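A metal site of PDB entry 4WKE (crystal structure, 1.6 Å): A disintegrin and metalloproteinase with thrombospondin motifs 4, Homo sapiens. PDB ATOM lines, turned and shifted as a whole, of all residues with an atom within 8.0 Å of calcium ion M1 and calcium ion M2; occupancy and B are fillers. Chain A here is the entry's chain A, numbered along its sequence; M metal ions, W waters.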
ATOM      1  N   PHE A   7      32.103 -22.415  -2.100  1.00  0.00           N
ATOM      2  CA  PHE A   7      30.933 -21.707  -1.601  1.00  0.00           C
ATOM      3  C   PHE A   7      30.564 -22.237  -0.227  1.00  0.00           C
ATOM      4  O   PHE A   7      30.379 -23.432  -0.058  1.00  0.00           O
ATOM      5  CB  PHE A   7      29.742 -21.919  -2.540  1.00  0.00           C
ATOM      6  CG  PHE A   7      30.047 -21.564  -3.956  1.00  0.00           C
ATOM      7  CD1 PHE A   7      30.493 -22.542  -4.842  1.00  0.00           C
ATOM      8  CD2 PHE A   7      29.928 -20.257  -4.411  1.00  0.00           C
ATOM      9  CE1 PHE A   7      30.797 -22.222  -6.155  1.00  0.00           C
ATOM     10  CE2 PHE A   7      30.232 -19.937  -5.724  1.00  0.00           C
ATOM     11  CZ  PHE A   7      30.675 -20.921  -6.588  1.00  0.00           C
ATOM     12  N   VAL A   8      30.437 -21.340   0.733  1.00  0.00           N
ATOM     13  CA  VAL A   8      29.969 -21.741   2.056  1.00  0.00           C
ATOM     14  C   VAL A   8      28.508 -21.365   2.205  1.00  0.00           C
ATOM     15  O   VAL A   8      28.191 -20.182   2.359  1.00  0.00           O
ATOM     16  CB  VAL A   8      30.768 -21.046   3.179  1.00  0.00           C
ATOM     17  CG1 VAL A   8      30.353 -21.588   4.532  1.00  0.00           C
ATOM     18  CG2 VAL A   8      32.259 -21.212   2.980  1.00  0.00           C
ATOM     19  N   GLU A   9      27.618 -22.354   2.172  1.00  0.00           N
ATOM     20  CA  GLU A   9      26.192 -22.116   2.336  1.00  0.00           C
ATOM     21  C   GLU A   9      25.904 -21.874   3.807  1.00  0.00           C
ATOM     22  O   GLU A   9      26.056 -22.765   4.646  1.00  0.00           O
ATOM     23  CB  GLU A   9      25.383 -23.294   1.806  1.00  0.00           C
ATOM     24  CG  GLU A   9      25.599 -23.542   0.323  1.00  0.00           C
ATOM     25  CD  GLU A   9      24.990 -24.856  -0.165  1.00  0.00           C
ATOM     26  OE1 GLU A   9      25.509 -25.917   0.192  1.00  0.00           O
ATOM     27  OE2 GLU A   9      23.995 -24.841  -0.930  1.00  0.00           O
ATOM     28  N   THR A  10      25.534 -20.642   4.134  1.00  0.00           N
ATOM     29  CA  THR A  10      25.517 -20.213   5.519  1.00  0.00           C
ATOM     30  C   THR A  10      24.111 -19.974   6.071  1.00  0.00           C
ATOM     31  O   THR A  10      23.289 -19.272   5.448  1.00  0.00           O
ATOM     32  CB  THR A  10      26.385 -18.957   5.694  1.00  0.00           C
ATOM     33  OG1 THR A  10      27.675 -19.200   5.111  1.00  0.00           O
ATOM     34  CG2 THR A  10      26.521 -18.581   7.159  1.00  0.00           C
ATOM     35  N   THR A  55      22.334 -18.394   2.825  1.00  0.00           N
ATOM     36  CA  THR A  55      21.250 -19.146   2.193  1.00  0.00           C
ATOM     37  C   THR A  55      20.007 -19.279   3.046  1.00  0.00           C
ATOM     38  O   THR A  55      18.924 -19.510   2.501  1.00  0.00           O
ATOM     39  CB  THR A  55      21.735 -20.540   1.785  1.00  0.00           C
ATOM     40  OG1 THR A  55      22.230 -21.219   2.956  1.00  0.00           O
ATOM     41  CG2 THR A  55      22.836 -20.429   0.742  1.00  0.00           C
ATOM     42  N   THR A  89      19.499 -30.575   7.022  1.00  0.00           N
ATOM     43  CA  THR A  89      19.085 -31.802   6.360  1.00  0.00           C
ATOM     44  C   THR A  89      20.282 -32.722   6.196  1.00  0.00           C
ATOM     45  O   THR A  89      21.431 -32.278   6.286  1.00  0.00           O
ATOM     46  CB  THR A  89      18.458 -31.509   4.989  1.00  0.00           C
ATOM     47  OG1 THR A  89      19.429 -30.834   4.174  1.00  0.00           O
ATOM     48  CG2 THR A  89      17.214 -30.658   5.122  1.00  0.00           C
ATOM     49  N   GLU A  91      21.604 -34.258   3.559  1.00  0.00           N
ATOM     50  CA  GLU A  91      22.381 -34.196   2.311  1.00  0.00           C
ATOM     51  C   GLU A  91      22.575 -32.783   1.765  1.00  0.00           C
ATOM     52  O   GLU A  91      21.630 -31.998   1.678  1.00  0.00           O
ATOM     53  CB  GLU A  91      21.696 -35.074   1.252  1.00  0.00           C
ATOM     54  CG  GLU A  91      21.556 -36.522   1.667  1.00  0.00           C
ATOM     55  CD  GLU A  91      22.890 -37.207   1.913  1.00  0.00           C
ATOM     56  OE1 GLU A  91      23.916 -36.736   1.363  1.00  0.00           O
ATOM     57  OE2 GLU A  91      22.930 -38.227   2.641  1.00  0.00           O
ATOM     58  N   ASP A  92      23.803 -32.491   1.350  1.00  0.00           N
ATOM     59  CA  ASP A  92      24.160 -31.169   0.817  1.00  0.00           C
ATOM     60  C   ASP A  92      23.427 -30.839  -0.482  1.00  0.00           C
ATOM     61  O   ASP A  92      23.279 -29.669  -0.831  1.00  0.00           O
ATOM     62  CB  ASP A  92      25.673 -31.073   0.625  1.00  0.00           C
ATOM     63  CG  ASP A  92      26.210 -29.646   0.671  1.00  0.00           C
ATOM     64  OD1 ASP A  92      25.448 -28.682   0.719  1.00  0.00           O
ATOM     65  OD2 ASP A  92      27.443 -29.503   0.673  1.00  0.00           O
ATOM     66  N   SER A  93      22.960 -31.860  -1.192  1.00  0.00           N
ATOM     67  CA  SER A  93      22.195 -31.638  -2.414  1.00  0.00           C
ATOM     68  C   SER A  93      20.763 -31.144  -2.175  1.00  0.00           C
ATOM     69  O   SER A  93      20.117 -30.648  -3.105  1.00  0.00           O
ATOM     70  CB  SER A  93      22.176 -32.914  -3.259  1.00  0.00           C
ATOM     71  OG  SER A  93      21.665 -34.006  -2.518  1.00  0.00           O
ATOM     72  N   ASP A  94      20.271 -31.287  -0.946  1.00  0.00           N
ATOM     73  CA  ASP A  94      18.984 -30.714  -0.546  1.00  0.00           C
ATOM     74  C   ASP A  94      19.172 -29.206  -0.442  1.00  0.00           C
ATOM     75  O   ASP A  94      20.109 -28.769   0.226  1.00  0.00           O
ATOM     76  CB  ASP A  94      18.579 -31.287   0.814  1.00  0.00           C
ATOM     77  CG  ASP A  94      17.210 -30.826   1.274  1.00  0.00           C
ATOM     78  OD1 ASP A  94      16.888 -29.617   1.182  1.00  0.00           O
ATOM     79  OD2 ASP A  94      16.453 -31.680   1.762  1.00  0.00           O
ATOM     80  N   PRO A  95      18.304 -28.407  -1.089  1.00  0.00           N
ATOM     81  CA  PRO A  95      18.476 -26.947  -1.087  1.00  0.00           C
ATOM     82  C   PRO A  95      18.433 -26.324   0.325  1.00  0.00           C
ATOM     83  O   PRO A  95      19.025 -25.255   0.516  1.00  0.00           O
ATOM     84  CB  PRO A  95      17.293 -26.444  -1.932  1.00  0.00           C
ATOM     85  CG  PRO A  95      16.286 -27.539  -1.875  1.00  0.00           C
ATOM     86  CD  PRO A  95      17.091 -28.808  -1.834  1.00  0.00           C
ATOM     87  N   ASP A  96      17.769 -26.969   1.275  1.00  0.00           N
ATOM     88  CA  ASP A  96      17.684 -26.460   2.652  1.00  0.00           C
ATOM     89  C   ASP A  96      18.955 -26.743   3.453  1.00  0.00           C
ATOM     90  O   ASP A  96      19.127 -26.234   4.572  1.00  0.00           O
ATOM     91  CB  ASP A  96      16.503 -27.076   3.423  1.00  0.00           C
ATOM     92  CG  ASP A  96      15.149 -26.621   2.913  1.00  0.00           C
ATOM     93  OD1 ASP A  96      15.049 -25.632   2.158  1.00  0.00           O
ATOM     94  OD2 ASP A  96      14.144 -27.272   3.302  1.00  0.00           O
ATOM     95  N   HIS A  97      19.847 -27.581   2.919  1.00  0.00           N
ATOM     96  CA  HIS A  97      21.071 -27.898   3.637  1.00  0.00           C
ATOM     97  C   HIS A  97      21.970 -26.686   3.719  1.00  0.00           C
ATOM     98  O   HIS A  97      22.049 -25.902   2.770  1.00  0.00           O
ATOM     99  CB  HIS A  97      21.832 -29.035   2.948  1.00  0.00           C
ATOM    100  CG  HIS A  97      23.024 -29.504   3.720  1.00  0.00           C
ATOM    101  ND1 HIS A  97      22.942 -30.475   4.693  1.00  0.00           N
ATOM    102  CD2 HIS A  97      24.323 -29.108   3.685  1.00  0.00           C
ATOM    103  CE1 HIS A  97      24.137 -30.672   5.217  1.00  0.00           C
ATOM    104  NE2 HIS A  97      24.996 -29.863   4.616  1.00  0.00           N
ATOM    105  N   PHE A  98      22.665 -26.547   4.843  1.00  0.00           N
ATOM    106  CA  PHE A  98      23.671 -25.487   4.992  1.00  0.00           C
ATOM    107  C   PHE A  98      24.982 -26.078   5.508  1.00  0.00           C
ATOM    108  O   PHE A  98      24.992 -27.143   6.139  1.00  0.00           O
ATOM    109  CB  PHE A  98      23.177 -24.354   5.909  1.00  0.00           C
ATOM    110  CG  PHE A  98      22.635 -24.811   7.229  1.00  0.00           C
ATOM    111  CD1 PHE A  98      23.456 -24.916   8.348  1.00  0.00           C
ATOM    112  CD2 PHE A  98      21.292 -25.139   7.373  1.00  0.00           C
ATOM    113  CE1 PHE A  98      22.948 -25.331   9.568  1.00  0.00           C
ATOM    114  CE2 PHE A  98      20.779 -25.532   8.585  1.00  0.00           C
ATOM    115  CZ  PHE A  98      21.616 -25.648   9.689  1.00  0.00           C
ATOM    116  N   ASP A  99      26.065 -25.392   5.182  1.00  0.00           N
ATOM    117  CA  ASP A  99      27.435 -25.824   5.523  1.00  0.00           C
ATOM    118  C   ASP A  99      27.974 -25.260   6.834  1.00  0.00           C
ATOM    119  O   ASP A  99      28.894 -25.847   7.426  1.00  0.00           O
ATOM    120  CB  ASP A  99      28.416 -25.414   4.412  1.00  0.00           C
ATOM    121  CG  ASP A  99      28.077 -25.985   3.045  1.00  0.00           C
ATOM    122  OD1 ASP A  99      27.708 -27.165   2.954  1.00  0.00           O
ATOM    123  OD2 ASP A  99      28.206 -25.256   2.048  1.00  0.00           O
ATOM    124  N   THR A 100      27.460 -24.120   7.279  1.00  0.00           N
ATOM    125  CA  THR A 100      27.889 -23.556   8.548  1.00  0.00           C
ATOM    126  C   THR A 100      26.760 -22.718   9.116  1.00  0.00           C
ATOM    127  O   THR A 100      25.880 -22.264   8.372  1.00  0.00           O
ATOM    128  CB  THR A 100      29.199 -22.743   8.395  1.00  0.00           C
ATOM    129  OG1 THR A 100      29.881 -22.666   9.654  1.00  0.00           O
ATOM    130  CG2 THR A 100      28.959 -21.368   7.831  1.00  0.00           C
ATOM    131  N   VAL A 126      34.395 -26.916   9.179  1.00  0.00           N
ATOM    132  CA  VAL A 126      33.451 -26.343   8.198  1.00  0.00           C
ATOM    133  C   VAL A 126      32.544 -27.372   7.526  1.00  0.00           C
ATOM    134  O   VAL A 126      31.387 -27.072   7.244  1.00  0.00           O
ATOM    135  CB  VAL A 126      34.145 -25.431   7.149  1.00  0.00           C
ATOM    136  CG1 VAL A 126      34.812 -26.234   6.035  1.00  0.00           C
ATOM    137  CG2 VAL A 126      33.147 -24.437   6.557  1.00  0.00           C
ATOM    138  N   CYS A 127      33.051 -28.566   7.256  1.00  0.00           N
ATOM    139  CA  CYS A 127      32.248 -29.588   6.576  1.00  0.00           C
ATOM    140  C   CYS A 127      31.815 -30.738   7.480  1.00  0.00           C
ATOM    141  O   CYS A 127      31.536 -31.840   7.016  1.00  0.00           O
ATOM    142  CB  CYS A 127      32.969 -30.100   5.327  1.00  0.00           C
ATOM    143  SG  CYS A 127      33.036 -28.834   4.051  1.00  0.00           S
ATOM    144  N   GLY A 209      37.312 -29.304   2.867  1.00  0.00           N
ATOM    145  CA  GLY A 209      36.293 -28.436   2.295  1.00  0.00           C
ATOM    146  C   GLY A 209      35.460 -29.115   1.225  1.00  0.00           C
ATOM    147  O   GLY A 209      34.964 -28.448   0.323  1.00  0.00           O
ATOM    148  N   HIS A 210      35.285 -30.422   1.334  1.00  0.00           N
ATOM    149  CA  HIS A 210      34.573 -31.206   0.319  1.00  0.00           C
ATOM    150  C   HIS A 210      33.105 -30.817   0.169  1.00  0.00           C
ATOM    151  O   HIS A 210      32.481 -31.128  -0.838  1.00  0.00           O
ATOM    152  CB  HIS A 210      34.667 -32.698   0.616  1.00  0.00           C
ATOM    153  CG  HIS A 210      34.143 -33.065   1.956  1.00  0.00           C
ATOM    154  ND1 HIS A 210      32.807 -33.292   2.207  1.00  0.00           N
ATOM    155  CD2 HIS A 210      34.769 -33.200   3.148  1.00  0.00           C
ATOM    156  CE1 HIS A 210      32.638 -33.569   3.486  1.00  0.00           C
ATOM    157  NE2 HIS A 210      33.817 -33.517   4.079  1.00  0.00           N
ATOM    158  N   CYS A 211      32.554 -30.133   1.173  1.00  0.00           N
ATOM    159  CA  CYS A 211      31.159 -29.701   1.140  1.00  0.00           C
ATOM    160  C   CYS A 211      30.999 -28.299   0.576  1.00  0.00           C
ATOM    161  O   CYS A 211      29.892 -27.775   0.562  1.00  0.00           O
ATOM    162  CB  CYS A 211      30.552 -29.761   2.538  1.00  0.00           C
ATOM    163  SG  CYS A 211      31.069 -28.435   3.644  1.00  0.00           S
ATOM    164  N   LEU A 212      32.086 -27.688   0.110  1.00  0.00           N
ATOM    165  CA  LEU A 212      32.041 -26.332  -0.362  1.00  0.00           C
ATOM    166  C   LEU A 212      32.049 -26.247  -1.876  1.00  0.00           C
ATOM    167  O   LEU A 212      32.223 -25.162  -2.452  1.00  0.00           O
ATOM    168  CB  LEU A 212      33.241 -25.561   0.187  1.00  0.00           C
ATOM    169  CG  LEU A 212      33.389 -25.585   1.702  1.00  0.00           C
ATOM    170  CD1 LEU A 212      34.661 -24.839   2.075  1.00  0.00           C
ATOM    171  CD2 LEU A 212      32.171 -24.987   2.407  1.00  0.00           C
ATOM    172  N   LEU A 213      31.832 -27.386  -2.546  1.00  0.00           N
ATOM    173  CA  LEU A 213      31.990 -27.427  -3.992  1.00  0.00           C
ATOM    174  C   LEU A 213      30.705 -27.184  -4.760  1.00  0.00           C
ATOM    175  O   LEU A 213      30.773 -26.870  -5.947  1.00  0.00           O
ATOM    176  CB  LEU A 213      32.618 -28.750  -4.425  1.00  0.00           C
ATOM    177  CG  LEU A 213      33.929 -29.159  -3.756  1.00  0.00           C
ATOM    178  CD1 LEU A 213      34.428 -30.470  -4.339  1.00  0.00           C
ATOM    179  CD2 LEU A 213      34.984 -28.083  -3.920  1.00  0.00           C
ATOM    180  N   ASP A 214      29.551 -27.359  -4.120  1.00  0.00           N
ATOM    181  CA  ASP A 214      28.268 -27.152  -4.776  1.00  0.00           C
ATOM    182  C   ASP A 214      27.819 -25.689  -4.686  1.00  0.00           C
ATOM    183  O   ASP A 214      27.995 -25.037  -3.665  1.00  0.00           O
ATOM    184  CB  ASP A 214      27.193 -28.118  -4.237  1.00  0.00           C
ATOM    185  CG  ASP A 214      26.877 -27.921  -2.750  1.00  0.00           C
ATOM    186  OD1 ASP A 214      27.797 -27.782  -1.916  1.00  0.00           O
ATOM    187  OD2 ASP A 214      25.675 -27.952  -2.412  1.00  0.00           O
ATOM    188  N   LYS A 215      27.276 -25.166  -5.778  1.00  0.00           N
ATOM    189  CA  LYS A 215      26.851 -23.775  -5.844  1.00  0.00           C
ATOM    190  C   LYS A 215      25.443 -23.652  -5.265  1.00  0.00           C
ATOM    191  O   LYS A 215      24.578 -24.469  -5.577  1.00  0.00           O
ATOM    192  CB  LYS A 215      26.885 -23.291  -7.304  1.00  0.00           C
ATOM    193  CG  LYS A 215      27.287 -21.838  -7.490  1.00  0.00           C
ATOM    194  CD  LYS A 215      27.943 -21.659  -8.854  1.00  0.00           C
ATOM    195  CE  LYS A 215      27.966 -20.215  -9.310  1.00  0.00           C
ATOM    196  NZ  LYS A 215      26.623 -19.762  -9.782  1.00  0.00           N
ATOM    197  N   PRO A 216      25.192 -22.643  -4.401  1.00  0.00           N
ATOM    198  CA  PRO A 216      23.841 -22.488  -3.857  1.00  0.00           C
ATOM    199  C   PRO A 216      22.845 -22.006  -4.900  1.00  0.00           C
ATOM    200  O   PRO A 216      23.201 -21.252  -5.802  1.00  0.00           O
ATOM    201  CB  PRO A 216      24.010 -21.436  -2.763  1.00  0.00           C
ATOM    202  CG  PRO A 216      25.249 -20.705  -3.130  1.00  0.00           C
ATOM    203  CD  PRO A 216      26.141 -21.724  -3.765  1.00  0.00           C
ATOM    204  N   GLU A 217      21.596 -22.433  -4.745  1.00  0.00           N
ATOM    205  CA  GLU A 217      20.527 -22.144  -5.715  1.00  0.00           C
ATOM    206  C   GLU A 217      19.908 -20.760  -5.530  1.00  0.00           C
ATOM    207  O   GLU A 217      19.546 -20.101  -6.510  1.00  0.00           O
ATOM    208  CB  GLU A 217      19.429 -23.204  -5.579  1.00  0.00           C
HETATM  209 CA    CA M   1      27.663 -27.037   0.430  1.00  0.00          CA
HETATM  210 CA    CA M   2      24.085 -27.434  -0.924  1.00  0.00          CA
HETATM  211  O   HOH W   1      28.455 -25.201  -0.944  1.00  0.00           O
HETATM  212  O   HOH W   2      22.889 -27.077  -2.945  1.00  0.00           O
HETATM  213  O   HOH W   3      22.084 -26.940   0.271  1.00  0.00           O
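Calcium ion M2 is bound by OD2 of Asp 214, 2.2 Å away.
The side-chain carboxylate (OE1) of Glu 9 binds calcium ion M2 (2.4 Å).
Water W2 is bound to calcium ion M2 (2.4 Å).
Calcium ion M2 is bound by O of Asp 92 (2.4 Å).
Water W3 binds calcium ion M2.
Calcium ion M2 is bound by OD1 of Asp 92.
Calcium ion M2 is bound by the side-chain carboxylate (OE2) of Glu 9.
Calcium ion M1 is bound by the backbone carbonyl oxygen (O) of Cys 211 (2.4 Å), water W1 (2.4 Å), the side-chain carboxylate (OE1) of Glu 9 (2.4 Å), the side-chain carboxylate (OD1) of Asp 214 (2.5 Å), the side-chain carboxylate (OD2) of Asp 99 (2.5 Å), the side-chain carboxylate (OD2) of Asp 92 (2.5 Å), the side-chain carboxylate (OD1) of Asp 99 (2.5 Å) and the side-chain carboxylate (OD1) of Asp 92 (2.8 Å).
Water W1 lies within hydrogen-bond range of O of Phe 7 (2.8 Å) and O of Asp 214 (2.8 Å).
Within 4 Å of calcium ion M1: Glu 9, Asp 92, Asp 99, Cys 211 and Asp 214.
Along chain A the residues within 4 Å of calcium ion M1 span positions 9 to 214.
The side-chain sulfur of Cys 211 forms a disulfide with the side-chain sulfur of Cys 127.
The backbone NH (N) of Thr 100 lies within hydrogen-bond range of the backbone carbonyl oxygen (O) of Glu 9.
Three residues have an atom within 4 Å of calcium ion M2: Glu 9, Asp 92 and Asp 214.
The nearest printed residue that does not touch calcium ion M2 is Asp 94 (4.3 Å).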
